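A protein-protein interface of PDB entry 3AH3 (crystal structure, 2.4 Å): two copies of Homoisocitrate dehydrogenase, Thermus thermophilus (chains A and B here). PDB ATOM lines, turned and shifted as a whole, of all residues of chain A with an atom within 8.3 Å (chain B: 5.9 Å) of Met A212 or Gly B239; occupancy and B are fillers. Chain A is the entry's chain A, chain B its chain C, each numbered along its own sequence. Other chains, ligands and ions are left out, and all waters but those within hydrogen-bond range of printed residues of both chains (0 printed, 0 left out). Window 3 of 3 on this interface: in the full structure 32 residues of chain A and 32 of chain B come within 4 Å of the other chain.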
ATOM      1  N   ARG A 109       7.036  15.254  22.863  1.00  0.00           N
ATOM      2  CA  ARG A 109       6.177  14.368  23.610  1.00  0.00           C
ATOM      3  C   ARG A 109       6.694  12.926  23.578  1.00  0.00           C
ATOM      4  O   ARG A 109       6.935  12.384  22.502  1.00  0.00           O
ATOM      5  CB  ARG A 109       4.774  14.448  23.036  1.00  0.00           C
ATOM      6  CG  ARG A 109       3.737  13.700  23.830  1.00  0.00           C
ATOM      7  CD  ARG A 109       2.383  14.235  23.500  1.00  0.00           C
ATOM      8  NE  ARG A 109       1.334  13.284  23.833  1.00  0.00           N
ATOM      9  CZ  ARG A 109       0.037  13.568  23.783  1.00  0.00           C
ATOM     10  NH1 ARG A 109      -0.371  14.782  23.426  1.00  0.00           N
ATOM     11  NH2 ARG A 109      -0.854  12.642  24.101  1.00  0.00           N
ATOM     12  N   ASN A 205     -11.411  11.323  13.461  1.00  0.00           N
ATOM     13  CA  ASN A 205     -11.157  10.626  14.723  1.00  0.00           C
ATOM     14  C   ASN A 205      -9.679  10.313  14.884  1.00  0.00           C
ATOM     15  O   ASN A 205      -9.159  10.276  15.996  1.00  0.00           O
ATOM     16  CB  ASN A 205     -11.960   9.324  14.801  1.00  0.00           C
ATOM     17  CG  ASN A 205     -13.447   9.559  14.843  1.00  0.00           C
ATOM     18  OD1 ASN A 205     -13.907  10.610  15.285  1.00  0.00           O
ATOM     19  ND2 ASN A 205     -14.215   8.580  14.379  1.00  0.00           N
ATOM     20  N   CYS A 206      -9.007  10.074  13.763  1.00  0.00           N
ATOM     21  CA  CYS A 206      -7.580   9.762  13.795  1.00  0.00           C
ATOM     22  C   CYS A 206      -6.806  10.948  14.355  1.00  0.00           C
ATOM     23  O   CYS A 206      -5.958  10.780  15.235  1.00  0.00           O
ATOM     24  CB  CYS A 206      -7.059   9.359  12.411  1.00  0.00           C
ATOM     25  SG  CYS A 206      -5.334   8.806  12.391  1.00  0.00           S
ATOM     26  N   ALA A 207      -7.130  12.141  13.862  1.00  0.00           N
ATOM     27  CA  ALA A 207      -6.528  13.394  14.328  1.00  0.00           C
ATOM     28  C   ALA A 207      -6.719  13.643  15.824  1.00  0.00           C
ATOM     29  O   ALA A 207      -5.771  14.018  16.513  1.00  0.00           O
ATOM     30  CB  ALA A 207      -7.071  14.566  13.531  1.00  0.00           C
ATOM     31  N   THR A 208      -7.937  13.431  16.327  1.00  0.00           N
ATOM     32  CA  THR A 208      -8.203  13.619  17.757  1.00  0.00           C
ATOM     33  C   THR A 208      -7.313  12.678  18.561  1.00  0.00           C
ATOM     34  O   THR A 208      -6.666  13.090  19.528  1.00  0.00           O
ATOM     35  CB  THR A 208      -9.697  13.404  18.129  1.00  0.00           C
ATOM     36  OG1 THR A 208     -10.533  14.140  17.234  1.00  0.00           O
ATOM     37  CG2 THR A 208      -9.978  13.895  19.526  1.00  0.00           C
ATOM     38  N   GLN A 209      -7.261  11.425  18.116  1.00  0.00           N
ATOM     39  CA  GLN A 209      -6.466  10.393  18.763  1.00  0.00           C
ATOM     40  C   GLN A 209      -4.969  10.650  18.703  1.00  0.00           C
ATOM     41  O   GLN A 209      -4.273  10.430  19.693  1.00  0.00           O
ATOM     42  CB  GLN A 209      -6.805   9.018  18.193  1.00  0.00           C
ATOM     43  CG  GLN A 209      -8.201   8.552  18.554  1.00  0.00           C
ATOM     44  CD  GLN A 209      -8.522   8.824  19.996  1.00  0.00           C
ATOM     45  OE1 GLN A 209      -7.849   8.327  20.900  1.00  0.00           O
ATOM     46  NE2 GLN A 209      -9.539   9.639  20.226  1.00  0.00           N
ATOM     47  N   LEU A 210      -4.468  11.118  17.564  1.00  0.00           N
ATOM     48  CA  LEU A 210      -3.051  11.474  17.475  1.00  0.00           C
ATOM     49  C   LEU A 210      -2.635  12.508  18.522  1.00  0.00           C
ATOM     50  O   LEU A 210      -1.499  12.495  18.989  1.00  0.00           O
ATOM     51  CB  LEU A 210      -2.682  11.953  16.071  1.00  0.00           C
ATOM     52  CG  LEU A 210      -2.640  10.853  15.009  1.00  0.00           C
ATOM     53  CD1 LEU A 210      -2.465  11.448  13.627  1.00  0.00           C
ATOM     54  CD2 LEU A 210      -1.542   9.839  15.322  1.00  0.00           C
ATOM     55  N   VAL A 211      -3.563  13.394  18.882  1.00  0.00           N
ATOM     56  CA  VAL A 211      -3.329  14.386  19.915  1.00  0.00           C
ATOM     57  C   VAL A 211      -3.431  13.741  21.298  1.00  0.00           C
ATOM     58  O   VAL A 211      -2.550  13.936  22.139  1.00  0.00           O
ATOM     59  CB  VAL A 211      -4.319  15.585  19.799  1.00  0.00           C
ATOM     60  CG1 VAL A 211      -4.115  16.584  20.933  1.00  0.00           C
ATOM     61  CG2 VAL A 211      -4.159  16.280  18.458  1.00  0.00           C
ATOM     62  N   MET A 212      -4.498  12.976  21.528  1.00  0.00           N
ATOM     63  CA  MET A 212      -4.752  12.393  22.853  1.00  0.00           C
ATOM     64  C   MET A 212      -3.885  11.163  23.112  1.00  0.00           C
ATOM     65  O   MET A 212      -3.202  11.095  24.124  1.00  0.00           O
ATOM     66  CB  MET A 212      -6.238  12.033  23.046  1.00  0.00           C
ATOM     67  CG  MET A 212      -7.229  13.155  22.724  1.00  0.00           C
ATOM     68  SD  MET A 212      -8.854  12.978  23.500  1.00  0.00           S
ATOM     69  CE  MET A 212      -9.613  11.691  22.532  1.00  0.00           C
ATOM     70  N   ARG A 213      -3.911  10.206  22.185  1.00  0.00           N
ATOM     71  CA  ARG A 213      -3.253   8.907  22.359  1.00  0.00           C
ATOM     72  C   ARG A 213      -2.385   8.501  21.160  1.00  0.00           C
ATOM     73  O   ARG A 213      -2.637   7.469  20.544  1.00  0.00           O
ATOM     74  CB  ARG A 213      -4.308   7.823  22.626  1.00  0.00           C
ATOM     75  CG  ARG A 213      -5.194   8.117  23.817  1.00  0.00           C
ATOM     76  CD  ARG A 213      -6.326   7.122  23.953  1.00  0.00           C
ATOM     77  NE  ARG A 213      -7.283   7.516  24.996  1.00  0.00           N
ATOM     78  CZ  ARG A 213      -8.423   8.169  24.771  1.00  0.00           C
ATOM     79  NH1 ARG A 213      -9.222   8.476  25.789  1.00  0.00           N
ATOM     80  NH2 ARG A 213      -8.776   8.512  23.534  1.00  0.00           N
ATOM     81  N   PRO A 214      -1.342   9.293  20.836  1.00  0.00           N
ATOM     82  CA  PRO A 214      -0.549   8.957  19.650  1.00  0.00           C
ATOM     83  C   PRO A 214       0.185   7.609  19.738  1.00  0.00           C
ATOM     84  O   PRO A 214       0.558   7.040  18.701  1.00  0.00           O
ATOM     85  CB  PRO A 214       0.456  10.109  19.562  1.00  0.00           C
ATOM     86  CG  PRO A 214       0.556  10.636  20.948  1.00  0.00           C
ATOM     87  CD  PRO A 214      -0.809  10.476  21.536  1.00  0.00           C
ATOM     88  N   GLU A 215       0.368   7.099  20.957  1.00  0.00           N
ATOM     89  CA  GLU A 215       1.124   5.857  21.188  1.00  0.00           C
ATOM     90  C   GLU A 215       0.479   4.578  20.628  1.00  0.00           C
ATOM     91  O   GLU A 215       1.159   3.557  20.490  1.00  0.00           O
ATOM     92  CB  GLU A 215       1.473   5.679  22.682  1.00  0.00           C
ATOM     93  CG  GLU A 215       0.270   5.605  23.642  1.00  0.00           C
ATOM     94  CD  GLU A 215      -0.300   6.981  24.016  1.00  0.00           C
ATOM     95  OE1 GLU A 215       0.302   8.020  23.653  1.00  0.00           O
ATOM     96  OE2 GLU A 215      -1.359   7.018  24.687  1.00  0.00           O
ATOM     97  N   ARG A 216      -0.811   4.622  20.305  1.00  0.00           N
ATOM     98  CA  ARG A 216      -1.478   3.434  19.754  1.00  0.00           C
ATOM     99  C   ARG A 216      -1.266   3.252  18.247  1.00  0.00           C
ATOM    100  O   ARG A 216      -1.632   2.221  17.683  1.00  0.00           O
ATOM    101  CB  ARG A 216      -2.973   3.374  20.122  1.00  0.00           C
ATOM    102  CG  ARG A 216      -3.841   4.424  19.475  1.00  0.00           C
ATOM    103  CD  ARG A 216      -5.332   4.054  19.517  1.00  0.00           C
ATOM    104  NE  ARG A 216      -5.978   4.371  20.793  1.00  0.00           N
ATOM    105  CZ  ARG A 216      -7.293   4.520  20.962  1.00  0.00           C
ATOM    106  NH1 ARG A 216      -7.778   4.797  22.167  1.00  0.00           N
ATOM    107  NH2 ARG A 216      -8.131   4.396  19.936  1.00  0.00           N
ATOM    108  N   TYR A 217      -0.657   4.240  17.604  1.00  0.00           N
ATOM    109  CA  TYR A 217      -0.464   4.172  16.165  1.00  0.00           C
ATOM    110  C   TYR A 217       0.951   3.832  15.796  1.00  0.00           C
ATOM    111  O   TYR A 217       1.902   4.218  16.472  1.00  0.00           O
ATOM    112  CB  TYR A 217      -0.906   5.469  15.480  1.00  0.00           C
ATOM    113  CG  TYR A 217      -2.354   5.763  15.736  1.00  0.00           C
ATOM    114  CD1 TYR A 217      -3.347   5.116  15.018  1.00  0.00           C
ATOM    115  CD2 TYR A 217      -2.734   6.659  16.732  1.00  0.00           C
ATOM    116  CE1 TYR A 217      -4.686   5.368  15.267  1.00  0.00           C
ATOM    117  CE2 TYR A 217      -4.064   6.916  16.989  1.00  0.00           C
ATOM    118  CZ  TYR A 217      -5.035   6.265  16.253  1.00  0.00           C
ATOM    119  OH  TYR A 217      -6.365   6.510  16.505  1.00  0.00           O
ATOM    120  N   LEU A 233       0.290  17.780  12.464  1.00  0.00           N
ATOM    121  CA  LEU A 233      -0.127  17.478  13.821  1.00  0.00           C
ATOM    122  C   LEU A 233       0.994  16.725  14.544  1.00  0.00           C
ATOM    123  O   LEU A 233       1.465  17.162  15.593  1.00  0.00           O
ATOM    124  CB  LEU A 233      -1.423  16.647  13.795  1.00  0.00           C
ATOM    125  CG  LEU A 233      -2.152  16.293  15.097  1.00  0.00           C
ATOM    126  CD1 LEU A 233      -3.526  15.707  14.795  1.00  0.00           C
ATOM    127  CD2 LEU A 233      -1.348  15.322  15.960  1.00  0.00           C
ATOM    128  N   LEU A 237       3.525  17.508  17.941  1.00  0.00           N
ATOM    129  CA  LEU A 237       3.860  16.691  19.108  1.00  0.00           C
ATOM    130  C   LEU A 237       5.371  16.602  19.320  1.00  0.00           C
ATOM    131  O   LEU A 237       5.846  16.489  20.446  1.00  0.00           O
ATOM    132  CB  LEU A 237       3.277  15.287  18.960  1.00  0.00           C
ATOM    133  CG  LEU A 237       1.769  15.153  18.742  1.00  0.00           C
ATOM    134  CD1 LEU A 237       1.466  13.807  18.092  1.00  0.00           C
ATOM    135  CD2 LEU A 237       0.970  15.336  20.048  1.00  0.00           C
ATOM    136  N   VAL B 105     -11.097  19.619  32.968  1.00  0.00           N
ATOM    137  CA  VAL B 105     -11.219  18.157  32.847  1.00  0.00           C
ATOM    138  C   VAL B 105      -9.852  17.509  32.589  1.00  0.00           C
ATOM    139  O   VAL B 105      -8.914  18.205  32.192  1.00  0.00           O
ATOM    140  CB  VAL B 105     -12.223  17.736  31.730  1.00  0.00           C
ATOM    141  CG1 VAL B 105     -13.663  18.000  32.164  1.00  0.00           C
ATOM    142  CG2 VAL B 105     -11.907  18.427  30.396  1.00  0.00           C
ATOM    143  N   PRO B 106      -9.726  16.180  32.826  1.00  0.00           N
ATOM    144  CA  PRO B 106      -8.463  15.488  32.536  1.00  0.00           C
ATOM    145  C   PRO B 106      -8.014  15.647  31.084  1.00  0.00           C
ATOM    146  O   PRO B 106      -8.844  15.604  30.163  1.00  0.00           O
ATOM    147  CB  PRO B 106      -8.778  14.012  32.842  1.00  0.00           C
ATOM    148  CG  PRO B 106     -10.273  13.935  32.984  1.00  0.00           C
ATOM    149  CD  PRO B 106     -10.684  15.276  33.492  1.00  0.00           C
ATOM    150  N   GLY B 107      -6.709  15.840  30.898  1.00  0.00           N
ATOM    151  CA  GLY B 107      -6.112  15.988  29.572  1.00  0.00           C
ATOM    152  C   GLY B 107      -6.661  17.176  28.805  1.00  0.00           C
ATOM    153  O   GLY B 107      -6.982  17.067  27.614  1.00  0.00           O
ATOM    154  N   SER B 108      -6.783  18.311  29.494  1.00  0.00           N
ATOM    155  CA  SER B 108      -7.226  19.548  28.864  1.00  0.00           C
ATOM    156  C   SER B 108      -6.182  20.646  29.004  1.00  0.00           C
ATOM    157  O   SER B 108      -5.805  21.034  30.121  1.00  0.00           O
ATOM    158  CB  SER B 108      -8.566  20.014  29.427  1.00  0.00           C
ATOM    159  OG  SER B 108      -9.058  21.119  28.690  1.00  0.00           O
ATOM    160  N   ALA B 235     -10.173  19.595  19.370  1.00  0.00           N
ATOM    161  CA  ALA B 235     -10.953  18.851  20.357  1.00  0.00           C
ATOM    162  C   ALA B 235     -10.071  17.876  21.127  1.00  0.00           C
ATOM    163  O   ALA B 235     -10.370  17.531  22.271  1.00  0.00           O
ATOM    164  CB  ALA B 235     -12.100  18.125  19.699  1.00  0.00           C
ATOM    165  N   GLY B 236      -8.979  17.451  20.489  1.00  0.00           N
ATOM    166  CA  GLY B 236      -7.982  16.586  21.118  1.00  0.00           C
ATOM    167  C   GLY B 236      -7.304  17.208  22.324  1.00  0.00           C
ATOM    168  O   GLY B 236      -6.895  16.513  23.240  1.00  0.00           O
ATOM    169  N   LEU B 237      -7.187  18.529  22.312  1.00  0.00           N
ATOM    170  CA  LEU B 237      -6.628  19.272  23.429  1.00  0.00           C
ATOM    171  C   LEU B 237      -7.641  19.427  24.562  1.00  0.00           C
ATOM    172  O   LEU B 237      -7.258  19.666  25.702  1.00  0.00           O
ATOM    173  CB  LEU B 237      -6.181  20.659  22.962  1.00  0.00           C
ATOM    174  CG  LEU B 237      -5.532  20.839  21.585  1.00  0.00           C
ATOM    175  CD1 LEU B 237      -5.659  22.283  21.145  1.00  0.00           C
ATOM    176  CD2 LEU B 237      -4.078  20.397  21.575  1.00  0.00           C
ATOM    177  N   MET B 238      -8.926  19.290  24.233  1.00  0.00           N
ATOM    178  CA  MET B 238     -10.036  19.552  25.153  1.00  0.00           C
ATOM    179  C   MET B 238     -10.557  18.289  25.842  1.00  0.00           C
ATOM    180  O   MET B 238     -11.583  18.329  26.531  1.00  0.00           O
ATOM    181  CB  MET B 238     -11.211  20.202  24.401  1.00  0.00           C
ATOM    182  CG  MET B 238     -10.953  21.565  23.766  1.00  0.00           C
ATOM    183  SD  MET B 238     -10.246  22.747  24.925  1.00  0.00           S
ATOM    184  CE  MET B 238      -8.615  23.000  24.217  1.00  0.00           C
ATOM    185  N   GLY B 239      -9.867  17.169  25.644  1.00  0.00           N
ATOM    186  CA  GLY B 239     -10.327  15.886  26.170  1.00  0.00           C
ATOM    187  C   GLY B 239     -11.385  15.190  25.322  1.00  0.00           C
ATOM    188  O   GLY B 239     -12.184  14.402  25.840  1.00  0.00           O
ATOM    189  N   GLY B 240     -11.398  15.481  24.023  1.00  0.00           N
ATOM    190  CA  GLY B 240     -12.254  14.759  23.085  1.00  0.00           C
ATOM    191  C   GLY B 240     -13.394  15.556  22.478  1.00  0.00           C
ATOM    192  O   GLY B 240     -13.603  16.727  22.807  1.00  0.00           O
ATOM    193  N   LEU B 241     -14.135  14.895  21.592  1.00  0.00           N
ATOM    194  CA  LEU B 241     -15.262  15.499  20.880  1.00  0.00           C
ATOM    195  C   LEU B 241     -16.554  15.502  21.708  1.00  0.00           C
ATOM    196  O   LEU B 241     -17.541  16.137  21.325  1.00  0.00           O
ATOM    197  CB  LEU B 241     -15.486  14.782  19.538  1.00  0.00           C
ATOM    198  CG  LEU B 241     -14.411  14.985  18.457  1.00  0.00           C
ATOM    199  CD1 LEU B 241     -14.337  13.801  17.495  1.00  0.00           C
ATOM    200  CD2 LEU B 241     -14.633  16.284  17.690  1.00  0.00           C
ATOM    201  N   GLY B 242     -16.531  14.809  22.845  1.00  0.00           N
ATOM    202  CA  GLY B 242     -17.722  14.613  23.667  1.00  0.00           C
ATOM    203  C   GLY B 242     -18.154  15.792  24.521  1.00  0.00           C
ATOM    204  O   GLY B 242     -19.209  15.747  25.163  1.00  0.00           O
ATOM    205  N   LEU B 243     -17.343  16.845  24.542  1.00  0.00           N
ATOM    206  CA  LEU B 243     -17.667  18.040  25.318  1.00  0.00           C
ATOM    207  C   LEU B 243     -17.907  19.246  24.406  1.00  0.00           C
ATOM    208  O   LEU B 243     -18.208  20.349  24.878  1.00  0.00           O
ATOM    209  CB  LEU B 243     -16.557  18.332  26.336  1.00  0.00           C
ATOM    210  CG  LEU B 243     -16.302  17.263  27.416  1.00  0.00           C
ATOM    211  CD1 LEU B 243     -14.837  17.237  27.867  1.00  0.00           C
ATOM    212  CD2 LEU B 243     -17.250  17.419  28.616  1.00  0.00           C
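Of chain B, only Gly B236 (3.4 Å), Gly B239 (3.8 Å) and Gly B240 (3.6 Å) come within 4 Å of Met A212. Gly B239 touches one residue of chain A. Printed residues of chain A within 4 Å of Leu B241: Asn A205 and Thr A208. Of the printed residues of chain B, Asn A205 touches Leu B241 (3.9 Å). Of the printed residues of chain B, Val A211 touches Gly B236 (3.5 Å) and Leu B237 (3.9 Å). Of the printed residues of chain A, Leu B237 touches Val A211. Printed residues of chain A within 4 Å of Gly B236: Thr A208, Val A211 and Met A212. Ser B108 touches none of the printed residues of chain A. The nearest residue of chain B that does not touch Met A212 is Ala B235 (5.0 Å). The nearest printed residue of chain A that does not touch Leu B237 is Met A212 (5.4 Å).
The backbone carbonyl oxygen (O) of Gly B107 lies within hydrogen-bond range of the backbone NH (N) of Gly B239 (3.5 Å). The backbone carbonyl oxygen (O) of Val A211 lies within hydrogen-bond range of the guanidinium group (NH1) of Arg A109 (2.7 Å). The guanidinium group of Arg A109 is in hydrogen-bond range of the backbone carbonyl oxygen of Met A212 (2.8 Å). The backbone NH (N) of Gly B240 sits at hydrogen-bond distance from the backbone carbonyl oxygen (O) of Ala B235, 2.9 Å away.
Hydrophobic or aromatic side chains of chain B that line the printed part of chain A: Leu B237 and Leu B241. Among the printed residues, 8 pairs touch across the chains. Among the printed residues, no Asp or Glu carboxylate lies within 4 Å of a Lys or Arg side-chain nitrogen of the other chain.
Among the printed residues, merely in contact across the chains: Met A212 with Gly B236 (3.4 Å), Val A211 with Gly B236 (3.5 Å), Thr A208 with Gly B236 (3.7 Å), Met A212 with Gly B239 (3.8 Å), Thr A208 with Leu B241 (3.8 Å), Val A211 with Leu B237 (3.9 Å) and Asn A205 with Leu B241 (3.9 Å).
Position printed for both chains: 237. Of the 8 pairs that touch across the chains among the printed residues, none has its exchanged pair printed and touching as well.
The side-chain sulfur of Met A212 is in hydrogen-bond range of the backbone NH of Gly B240.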
